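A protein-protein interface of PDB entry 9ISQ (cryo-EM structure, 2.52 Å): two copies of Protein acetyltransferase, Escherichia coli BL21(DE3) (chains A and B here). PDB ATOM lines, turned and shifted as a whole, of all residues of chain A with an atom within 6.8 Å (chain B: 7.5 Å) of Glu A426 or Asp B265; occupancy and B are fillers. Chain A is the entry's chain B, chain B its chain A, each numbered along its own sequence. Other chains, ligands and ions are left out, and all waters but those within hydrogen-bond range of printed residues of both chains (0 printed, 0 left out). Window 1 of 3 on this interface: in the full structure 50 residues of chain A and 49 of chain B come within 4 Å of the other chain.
The side-chain hydroxyl (OG1) of Thr B266 is in hydrogen-bond range of the side-chain hydroxyl (OG1) of Thr A424, at 3.4 Å.
OD1 of Asp B265 sits close to N of Glu B268, at 3.4 Å. The backbone carbonyl oxygen (O) of Glu A426 is in hydrogen-bond range of the side-chain hydroxyl (OG1) of Thr A430, at 2.8 Å.
Thr B266 touches Leu A299 (CG2 to CD1, 3.8 Å). ND1 of His B267 touches CG2 of Thr A424, at 3.4 Å. Asp B265 touches Glu A426.
Printed residues of chain B within 4 Å of Leu A299: Thr B266 (3.8 Å). Ala A303 touches none of the printed residues of chain B. Of the printed residues of chain B, Thr A424 touches Thr B266 and His B267. Of the printed residues of chain B, Glu A426 touches Asp B265 (3.2 Å). Val B228 touches none of the printed residues of chain A. Of chain A, only Glu A426 (3.2 Å) comes within 4 Å of Asp B265. Of the printed residues of chain A, Thr B266 touches Leu A299 (3.8 Å) and Thr A424 (3.4 Å). Of the printed residues of chain A, His B267 touches Thr A424 (3.4 Å). The nearest residue of chain B that does not touch Glu A426 is Thr B266 (4.4 Å). The nearest residue of chain A that does not touch Asp B265 is Leu A299 (5.4 Å). The nearest printed residue of chain B that does not touch Leu A299 is Ile B229 (5.1 Å).
Along chain A the printed residues that touch a printed residue of chain B span positions 299 to 426. Among the printed residues, 4 pairs touch across the chains.
No position is printed for both chains. Of the 4 pairs that touch across the chains among the printed residues, none has its exchanged pair printed and touching as well.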
ATOM      1  N   PRO A 296      18.282 -19.685  11.264  1.00  0.00           N
ATOM      2  CA  PRO A 296      17.931 -20.754  10.317  1.00  0.00           C
ATOM      3  C   PRO A 296      17.891 -22.122  10.967  1.00  0.00           C
ATOM      4  O   PRO A 296      16.868 -22.814  10.887  1.00  0.00           O
ATOM      5  CB  PRO A 296      19.034 -20.658   9.256  1.00  0.00           C
ATOM      6  CG  PRO A 296      19.555 -19.286   9.366  1.00  0.00           C
ATOM      7  CD  PRO A 296      19.428 -18.890  10.794  1.00  0.00           C
ATOM      8  N   LEU A 299      14.840 -22.534  12.998  1.00  0.00           N
ATOM      9  CA  LEU A 299      13.661 -22.795  12.181  1.00  0.00           C
ATOM     10  C   LEU A 299      13.623 -24.248  11.738  1.00  0.00           C
ATOM     11  O   LEU A 299      12.545 -24.838  11.611  1.00  0.00           O
ATOM     12  CB  LEU A 299      13.642 -21.866  10.972  1.00  0.00           C
ATOM     13  CG  LEU A 299      13.416 -20.390  11.290  1.00  0.00           C
ATOM     14  CD1 LEU A 299      13.953 -19.512  10.172  1.00  0.00           C
ATOM     15  CD2 LEU A 299      11.944 -20.110  11.527  1.00  0.00           C
ATOM     16  N   ALA A 300      14.791 -24.844  11.498  1.00  0.00           N
ATOM     17  CA  ALA A 300      14.828 -26.257  11.150  1.00  0.00           C
ATOM     18  C   ALA A 300      14.427 -27.115  12.342  1.00  0.00           C
ATOM     19  O   ALA A 300      13.599 -28.025  12.214  1.00  0.00           O
ATOM     20  CB  ALA A 300      16.220 -26.635  10.650  1.00  0.00           C
ATOM     21  N   LEU A 301      14.970 -26.810  13.524  1.00  0.00           N
ATOM     22  CA  LEU A 301      14.744 -27.666  14.684  1.00  0.00           C
ATOM     23  C   LEU A 301      13.260 -27.835  14.955  1.00  0.00           C
ATOM     24  O   LEU A 301      12.766 -28.960  15.092  1.00  0.00           O
ATOM     25  CB  LEU A 301      15.449 -27.082  15.906  1.00  0.00           C
ATOM     26  CG  LEU A 301      16.976 -27.144  15.911  1.00  0.00           C
ATOM     27  CD1 LEU A 301      17.509 -26.553  17.200  1.00  0.00           C
ATOM     28  CD2 LEU A 301      17.465 -28.570  15.741  1.00  0.00           C
ATOM     29  N   ASP A 302      12.524 -26.723  14.999  1.00  0.00           N
ATOM     30  CA  ASP A 302      11.085 -26.795  15.229  1.00  0.00           C
ATOM     31  C   ASP A 302      10.434 -27.776  14.266  1.00  0.00           C
ATOM     32  O   ASP A 302       9.653 -28.641  14.675  1.00  0.00           O
ATOM     33  CB  ASP A 302      10.463 -25.408  15.083  1.00  0.00           C
ATOM     34  CG  ASP A 302      10.861 -24.469  16.202  1.00  0.00           C
ATOM     35  OD1 ASP A 302      11.229 -24.956  17.289  1.00  0.00           O
ATOM     36  OD2 ASP A 302      10.798 -23.238  15.998  1.00  0.00           O
ATOM     37  N   ALA A 303      10.774 -27.678  12.981  1.00  0.00           N
ATOM     38  CA  ALA A 303      10.201 -28.600  12.011  1.00  0.00           C
ATOM     39  C   ALA A 303      10.559 -30.038  12.360  1.00  0.00           C
ATOM     40  O   ALA A 303       9.686 -30.912  12.421  1.00  0.00           O
ATOM     41  CB  ALA A 303      10.680 -28.245  10.606  1.00  0.00           C
ATOM     42  N   LEU A 304      11.841 -30.296  12.629  1.00  0.00           N
ATOM     43  CA  LEU A 304      12.250 -31.637  13.026  1.00  0.00           C
ATOM     44  C   LEU A 304      11.595 -32.058  14.333  1.00  0.00           C
ATOM     45  O   LEU A 304      11.457 -33.259  14.589  1.00  0.00           O
ATOM     46  CB  LEU A 304      13.772 -31.708  13.155  1.00  0.00           C
ATOM     47  CG  LEU A 304      14.367 -33.105  13.325  1.00  0.00           C
ATOM     48  CD1 LEU A 304      14.316 -33.870  12.023  1.00  0.00           C
ATOM     49  CD2 LEU A 304      15.789 -33.012  13.830  1.00  0.00           C
ATOM     50  N   ARG A 307       7.926 -33.612  13.671  1.00  0.00           N
ATOM     51  CA  ARG A 307       7.846 -34.923  13.041  1.00  0.00           C
ATOM     52  C   ARG A 307       8.599 -35.987  13.831  1.00  0.00           C
ATOM     53  O   ARG A 307       8.835 -37.082  13.306  1.00  0.00           O
ATOM     54  CB  ARG A 307       8.385 -34.855  11.612  1.00  0.00           C
ATOM     55  CG  ARG A 307       7.383 -34.331  10.603  1.00  0.00           C
ATOM     56  CD  ARG A 307       8.010 -34.191   9.232  1.00  0.00           C
ATOM     57  NE  ARG A 307       8.169 -32.793   8.846  1.00  0.00           N
ATOM     58  CZ  ARG A 307       7.409 -32.155   7.965  1.00  0.00           C
ATOM     59  NH1 ARG A 307       6.409 -32.762   7.340  1.00  0.00           N
ATOM     60  NH2 ARG A 307       7.659 -30.877   7.699  1.00  0.00           N
ATOM     61  N   MET A 364      23.649 -31.592   7.070  1.00  0.00           N
ATOM     62  CA  MET A 364      22.893 -30.497   6.474  1.00  0.00           C
ATOM     63  C   MET A 364      23.666 -29.206   6.690  1.00  0.00           C
ATOM     64  O   MET A 364      23.902 -28.802   7.835  1.00  0.00           O
ATOM     65  CB  MET A 364      21.490 -30.420   7.083  1.00  0.00           C
ATOM     66  CG  MET A 364      20.801 -29.069   6.977  1.00  0.00           C
ATOM     67  SD  MET A 364      19.191 -29.081   7.782  1.00  0.00           S
ATOM     68  CE  MET A 364      18.329 -27.827   6.847  1.00  0.00           C
ATOM     69  N   ASN A 400      21.768 -26.051   1.575  1.00  0.00           N
ATOM     70  CA  ASN A 400      20.737 -25.014   1.564  1.00  0.00           C
ATOM     71  C   ASN A 400      21.428 -23.654   1.542  1.00  0.00           C
ATOM     72  O   ASN A 400      21.811 -23.133   2.591  1.00  0.00           O
ATOM     73  CB  ASN A 400      19.817 -25.149   2.767  1.00  0.00           C
ATOM     74  CG  ASN A 400      18.689 -24.144   2.749  1.00  0.00           C
ATOM     75  OD1 ASN A 400      18.293 -23.659   1.693  1.00  0.00           O
ATOM     76  ND2 ASN A 400      18.172 -23.816   3.923  1.00  0.00           N
ATOM     77  N   THR A 424      14.709 -23.500   1.002  1.00  0.00           N
ATOM     78  CA  THR A 424      14.444 -22.990   2.335  1.00  0.00           C
ATOM     79  C   THR A 424      14.752 -24.049   3.383  1.00  0.00           C
ATOM     80  O   THR A 424      14.769 -25.243   3.075  1.00  0.00           O
ATOM     81  CB  THR A 424      12.975 -22.547   2.455  1.00  0.00           C
ATOM     82  OG1 THR A 424      12.836 -21.573   3.495  1.00  0.00           O
ATOM     83  CG2 THR A 424      12.062 -23.728   2.746  1.00  0.00           C
ATOM     84  N   PRO A 425      15.010 -23.643   4.625  1.00  0.00           N
ATOM     85  CA  PRO A 425      15.088 -24.625   5.708  1.00  0.00           C
ATOM     86  C   PRO A 425      13.707 -25.160   6.038  1.00  0.00           C
ATOM     87  O   PRO A 425      12.688 -24.527   5.769  1.00  0.00           O
ATOM     88  CB  PRO A 425      15.684 -23.842   6.883  1.00  0.00           C
ATOM     89  CG  PRO A 425      15.841 -22.437   6.427  1.00  0.00           C
ATOM     90  CD  PRO A 425      15.142 -22.268   5.126  1.00  0.00           C
ATOM     91  N   GLU A 426      13.692 -26.356   6.616  1.00  0.00           N
ATOM     92  CA  GLU A 426      12.513 -27.199   6.810  1.00  0.00           C
ATOM     93  C   GLU A 426      11.819 -27.548   5.498  1.00  0.00           C
ATOM     94  O   GLU A 426      10.710 -28.094   5.518  1.00  0.00           O
ATOM     95  CB  GLU A 426      11.495 -26.596   7.795  1.00  0.00           C
ATOM     96  CG  GLU A 426      10.648 -25.428   7.318  1.00  0.00           C
ATOM     97  CD  GLU A 426      10.970 -24.142   8.049  1.00  0.00           C
ATOM     98  OE1 GLU A 426      12.119 -23.667   7.968  1.00  0.00           O
ATOM     99  OE2 GLU A 426      10.067 -23.602   8.717  1.00  0.00           O
ATOM    100  N   GLY A 427      12.433 -27.244   4.360  1.00  0.00           N
ATOM    101  CA  GLY A 427      12.117 -27.924   3.124  1.00  0.00           C
ATOM    102  C   GLY A 427      13.073 -29.085   2.973  1.00  0.00           C
ATOM    103  O   GLY A 427      12.772 -30.088   2.322  1.00  0.00           O
ATOM    104  N   THR A 428      14.251 -28.941   3.586  1.00  0.00           N
ATOM    105  CA  THR A 428      15.205 -30.037   3.687  1.00  0.00           C
ATOM    106  C   THR A 428      14.762 -31.063   4.724  1.00  0.00           C
ATOM    107  O   THR A 428      14.863 -32.275   4.492  1.00  0.00           O
ATOM    108  CB  THR A 428      16.589 -29.486   4.044  1.00  0.00           C
ATOM    109  OG1 THR A 428      16.842 -28.288   3.301  1.00  0.00           O
ATOM    110  CG2 THR A 428      17.669 -30.497   3.732  1.00  0.00           C
ATOM    111  N   ILE A 429      14.264 -30.599   5.871  1.00  0.00           N
ATOM    112  CA  ILE A 429      13.819 -31.527   6.904  1.00  0.00           C
ATOM    113  C   ILE A 429      12.635 -32.342   6.408  1.00  0.00           C
ATOM    114  O   ILE A 429      12.488 -33.520   6.750  1.00  0.00           O
ATOM    115  CB  ILE A 429      13.475 -30.770   8.200  1.00  0.00           C
ATOM    116  CG1 ILE A 429      14.706 -30.053   8.753  1.00  0.00           C
ATOM    117  CG2 ILE A 429      12.909 -31.726   9.233  1.00  0.00           C
ATOM    118  CD1 ILE A 429      15.806 -30.975   9.221  1.00  0.00           C
ATOM    119  N   THR A 430      11.767 -31.731   5.604  1.00  0.00           N
ATOM    120  CA  THR A 430      10.632 -32.467   5.065  1.00  0.00           C
ATOM    121  C   THR A 430      11.104 -33.642   4.217  1.00  0.00           C
ATOM    122  O   THR A 430      10.602 -34.760   4.354  1.00  0.00           O
ATOM    123  CB  THR A 430       9.742 -31.533   4.246  1.00  0.00           C
ATOM    124  OG1 THR A 430       9.275 -30.467   5.079  1.00  0.00           O
ATOM    125  CG2 THR A 430       8.551 -32.282   3.688  1.00  0.00           C
ATOM    126  N   ALA A 431      12.089 -33.410   3.347  1.00  0.00           N
ATOM    127  CA  ALA A 431      12.623 -34.491   2.523  1.00  0.00           C
ATOM    128  C   ALA A 431      13.311 -35.554   3.371  1.00  0.00           C
ATOM    129  O   ALA A 431      13.146 -36.761   3.127  1.00  0.00           O
ATOM    130  CB  ALA A 431      13.592 -33.923   1.491  1.00  0.00           C
ATOM    131  N   VAL B 228       3.524 -10.719  12.520  1.00  0.00           N
ATOM    132  CA  VAL B 228       4.546 -11.188  13.443  1.00  0.00           C
ATOM    133  C   VAL B 228       4.998 -12.581  13.033  1.00  0.00           C
ATOM    134  O   VAL B 228       4.337 -13.278  12.264  1.00  0.00           O
ATOM    135  CB  VAL B 228       4.044 -11.206  14.904  1.00  0.00           C
ATOM    136  CG1 VAL B 228       5.208 -11.298  15.871  1.00  0.00           C
ATOM    137  CG2 VAL B 228       3.209  -9.979  15.195  1.00  0.00           C
ATOM    138  N   ILE B 229       6.156 -12.973  13.553  1.00  0.00           N
ATOM    139  CA  ILE B 229       6.622 -14.354  13.491  1.00  0.00           C
ATOM    140  C   ILE B 229       7.500 -14.600  14.709  1.00  0.00           C
ATOM    141  O   ILE B 229       8.361 -13.779  15.039  1.00  0.00           O
ATOM    142  CB  ILE B 229       7.383 -14.664  12.183  1.00  0.00           C
ATOM    143  CG1 ILE B 229       8.066 -16.027  12.278  1.00  0.00           C
ATOM    144  CG2 ILE B 229       8.412 -13.599  11.882  1.00  0.00           C
ATOM    145  CD1 ILE B 229       8.262 -16.698  10.943  1.00  0.00           C
ATOM    146  N   LYS B 230       7.267 -15.721  15.389  1.00  0.00           N
ATOM    147  CA  LYS B 230       8.022 -16.108  16.571  1.00  0.00           C
ATOM    148  C   LYS B 230       8.525 -17.533  16.401  1.00  0.00           C
ATOM    149  O   LYS B 230       7.909 -18.342  15.704  1.00  0.00           O
ATOM    150  CB  LYS B 230       7.174 -16.003  17.835  1.00  0.00           C
ATOM    151  CG  LYS B 230       7.983 -16.078  19.105  1.00  0.00           C
ATOM    152  CD  LYS B 230       7.237 -15.490  20.280  1.00  0.00           C
ATOM    153  CE  LYS B 230       8.044 -15.639  21.552  1.00  0.00           C
ATOM    154  NZ  LYS B 230       7.944 -17.010  22.118  1.00  0.00           N
ATOM    155  N   ARG B 262      -0.322 -13.698  12.904  1.00  0.00           N
ATOM    156  CA  ARG B 262       0.834 -14.561  13.106  1.00  0.00           C
ATOM    157  C   ARG B 262       1.029 -15.461  11.896  1.00  0.00           C
ATOM    158  O   ARG B 262       0.058 -15.958  11.320  1.00  0.00           O
ATOM    159  CB  ARG B 262       0.664 -15.414  14.366  1.00  0.00           C
ATOM    160  CG  ARG B 262       1.935 -16.107  14.811  1.00  0.00           C
ATOM    161  CD  ARG B 262       1.738 -16.889  16.095  1.00  0.00           C
ATOM    162  NE  ARG B 262       2.996 -17.438  16.591  1.00  0.00           N
ATOM    163  CZ  ARG B 262       3.155 -17.995  17.783  1.00  0.00           C
ATOM    164  NH1 ARG B 262       2.147 -18.118  18.628  1.00  0.00           N
ATOM    165  NH2 ARG B 262       4.355 -18.444  18.134  1.00  0.00           N
ATOM    166  N   VAL B 263       2.288 -15.666  11.509  1.00  0.00           N
ATOM    167  CA  VAL B 263       2.646 -16.574  10.426  1.00  0.00           C
ATOM    168  C   VAL B 263       3.565 -17.651  10.983  1.00  0.00           C
ATOM    169  O   VAL B 263       4.254 -17.449  11.986  1.00  0.00           O
ATOM    170  CB  VAL B 263       3.315 -15.845   9.240  1.00  0.00           C
ATOM    171  CG1 VAL B 263       2.398 -14.761   8.702  1.00  0.00           C
ATOM    172  CG2 VAL B 263       4.649 -15.263   9.646  1.00  0.00           C
ATOM    173  N   GLN B 264       3.578 -18.803  10.314  1.00  0.00           N
ATOM    174  CA  GLN B 264       4.232 -19.996  10.846  1.00  0.00           C
ATOM    175  C   GLN B 264       5.715 -20.060  10.491  1.00  0.00           C
ATOM    176  O   GLN B 264       6.571 -20.064  11.379  1.00  0.00           O
ATOM    177  CB  GLN B 264       3.524 -21.253  10.327  1.00  0.00           C
ATOM    178  CG  GLN B 264       2.063 -21.397  10.746  1.00  0.00           C
ATOM    179  CD  GLN B 264       1.806 -20.973  12.176  1.00  0.00           C
ATOM    180  OE1 GLN B 264       2.175 -21.672  13.117  1.00  0.00           O
ATOM    181  NE2 GLN B 264       1.161 -19.826  12.347  1.00  0.00           N
ATOM    182  N   ASP B 265       6.030 -20.111   9.200  1.00  0.00           N
ATOM    183  CA  ASP B 265       7.386 -20.362   8.731  1.00  0.00           C
ATOM    184  C   ASP B 265       7.804 -19.263   7.764  1.00  0.00           C
ATOM    185  O   ASP B 265       7.044 -18.336   7.471  1.00  0.00           O
ATOM    186  CB  ASP B 265       7.490 -21.736   8.058  1.00  0.00           C
ATOM    187  CG  ASP B 265       6.506 -21.900   6.924  1.00  0.00           C
ATOM    188  OD1 ASP B 265       5.726 -20.959   6.675  1.00  0.00           O
ATOM    189  OD2 ASP B 265       6.509 -22.966   6.275  1.00  0.00           O
ATOM    190  N   THR B 266       9.032 -19.376   7.264  1.00  0.00           N
ATOM    191  CA  THR B 266       9.558 -18.408   6.315  1.00  0.00           C
ATOM    192  C   THR B 266       9.056 -18.636   4.898  1.00  0.00           C
ATOM    193  O   THR B 266       9.212 -17.747   4.054  1.00  0.00           O
ATOM    194  CB  THR B 266      11.089 -18.442   6.319  1.00  0.00           C
ATOM    195  OG1 THR B 266      11.545 -19.779   6.078  1.00  0.00           O
ATOM    196  CG2 THR B 266      11.636 -17.938   7.652  1.00  0.00           C
ATOM    197  N   HIS B 267       8.453 -19.791   4.613  1.00  0.00           N
ATOM    198  CA  HIS B 267       7.939 -20.015   3.269  1.00  0.00           C
ATOM    199  C   HIS B 267       6.721 -19.140   3.010  1.00  0.00           C
ATOM    200  O   HIS B 267       6.502 -18.697   1.879  1.00  0.00           O
ATOM    201  CB  HIS B 267       7.565 -21.479   3.069  1.00  0.00           C
ATOM    202  CG  HIS B 267       7.909 -21.999   1.710  1.00  0.00           C
ATOM    203  ND1 HIS B 267       9.022 -22.775   1.480  1.00  0.00           N
ATOM    204  CD2 HIS B 267       7.356 -21.774   0.499  1.00  0.00           C
ATOM    205  CE1 HIS B 267       9.104 -23.063   0.197  1.00  0.00           C
ATOM    206  NE2 HIS B 267       8.111 -22.457  -0.424  1.00  0.00           N
ATOM    207  N   GLU B 268       5.919 -18.899   4.040  1.00  0.00           N
ATOM    208  CA  GLU B 268       4.832 -17.938   3.981  1.00  0.00           C
ATOM    209  C   GLU B 268       5.313 -16.514   4.201  1.00  0.00           C
ATOM    210  O   GLU B 268       4.496 -15.589   4.172  1.00  0.00           O
ATOM    211  CB  GLU B 268       3.777 -18.278   5.033  1.00  0.00           C
ATOM    212  CG  GLU B 268       3.273 -19.701   4.972  1.00  0.00           C
ATOM    213  CD  GLU B 268       2.388 -20.046   6.148  1.00  0.00           C
ATOM    214  OE1 GLU B 268       2.568 -19.435   7.221  1.00  0.00           O
ATOM    215  OE2 GLU B 268       1.516 -20.927   6.002  1.00  0.00           O
ATOM    216  N   LEU B 269       6.612 -16.320   4.432  1.00  0.00           N
ATOM    217  CA  LEU B 269       7.121 -14.988   4.708  1.00  0.00           C
ATOM    218  C   LEU B 269       7.415 -14.219   3.425  1.00  0.00           C
ATOM    219  O   LEU B 269       7.140 -13.018   3.358  1.00  0.00           O
ATOM    220  CB  LEU B 269       8.369 -15.074   5.584  1.00  0.00           C
ATOM    221  CG  LEU B 269       8.892 -13.750   6.147  1.00  0.00           C
ATOM    222  CD1 LEU B 269       7.881 -13.094   7.070  1.00  0.00           C
ATOM    223  CD2 LEU B 269      10.198 -13.975   6.871  1.00  0.00           C
ATOM    224  N   PHE B 270       7.964 -14.866   2.389  1.00  0.00           N
ATOM    225  CA  PHE B 270       8.093 -14.127   1.137  1.00  0.00           C
ATOM    226  C   PHE B 270       6.751 -13.959   0.443  1.00  0.00           C
ATOM    227  O   PHE B 270       6.565 -12.980  -0.286  1.00  0.00           O
ATOM    228  CB  PHE B 270       9.103 -14.740   0.155  1.00  0.00           C
ATOM    229  CG  PHE B 270       9.326 -16.216   0.289  1.00  0.00           C
ATOM    230  CD1 PHE B 270       8.354 -17.122  -0.085  1.00  0.00           C
ATOM    231  CD2 PHE B 270      10.560 -16.694   0.692  1.00  0.00           C
ATOM    232  CE1 PHE B 270       8.589 -18.481   0.007  1.00  0.00           C
ATOM    233  CE2 PHE B 270      10.803 -18.043   0.783  1.00  0.00           C
ATOM    234  CZ  PHE B 270       9.820 -18.940   0.439  1.00  0.00           C
ATOM    235  N   ALA B 272       4.286 -13.174   2.274  1.00  0.00           N
ATOM    236  CA  ALA B 272       3.894 -11.985   3.024  1.00  0.00           C
ATOM    237  C   ALA B 272       4.541 -10.732   2.451  1.00  0.00           C
ATOM    238  O   ALA B 272       3.916  -9.667   2.404  1.00  0.00           O
ATOM    239  CB  ALA B 272       4.265 -12.152   4.496  1.00  0.00           C
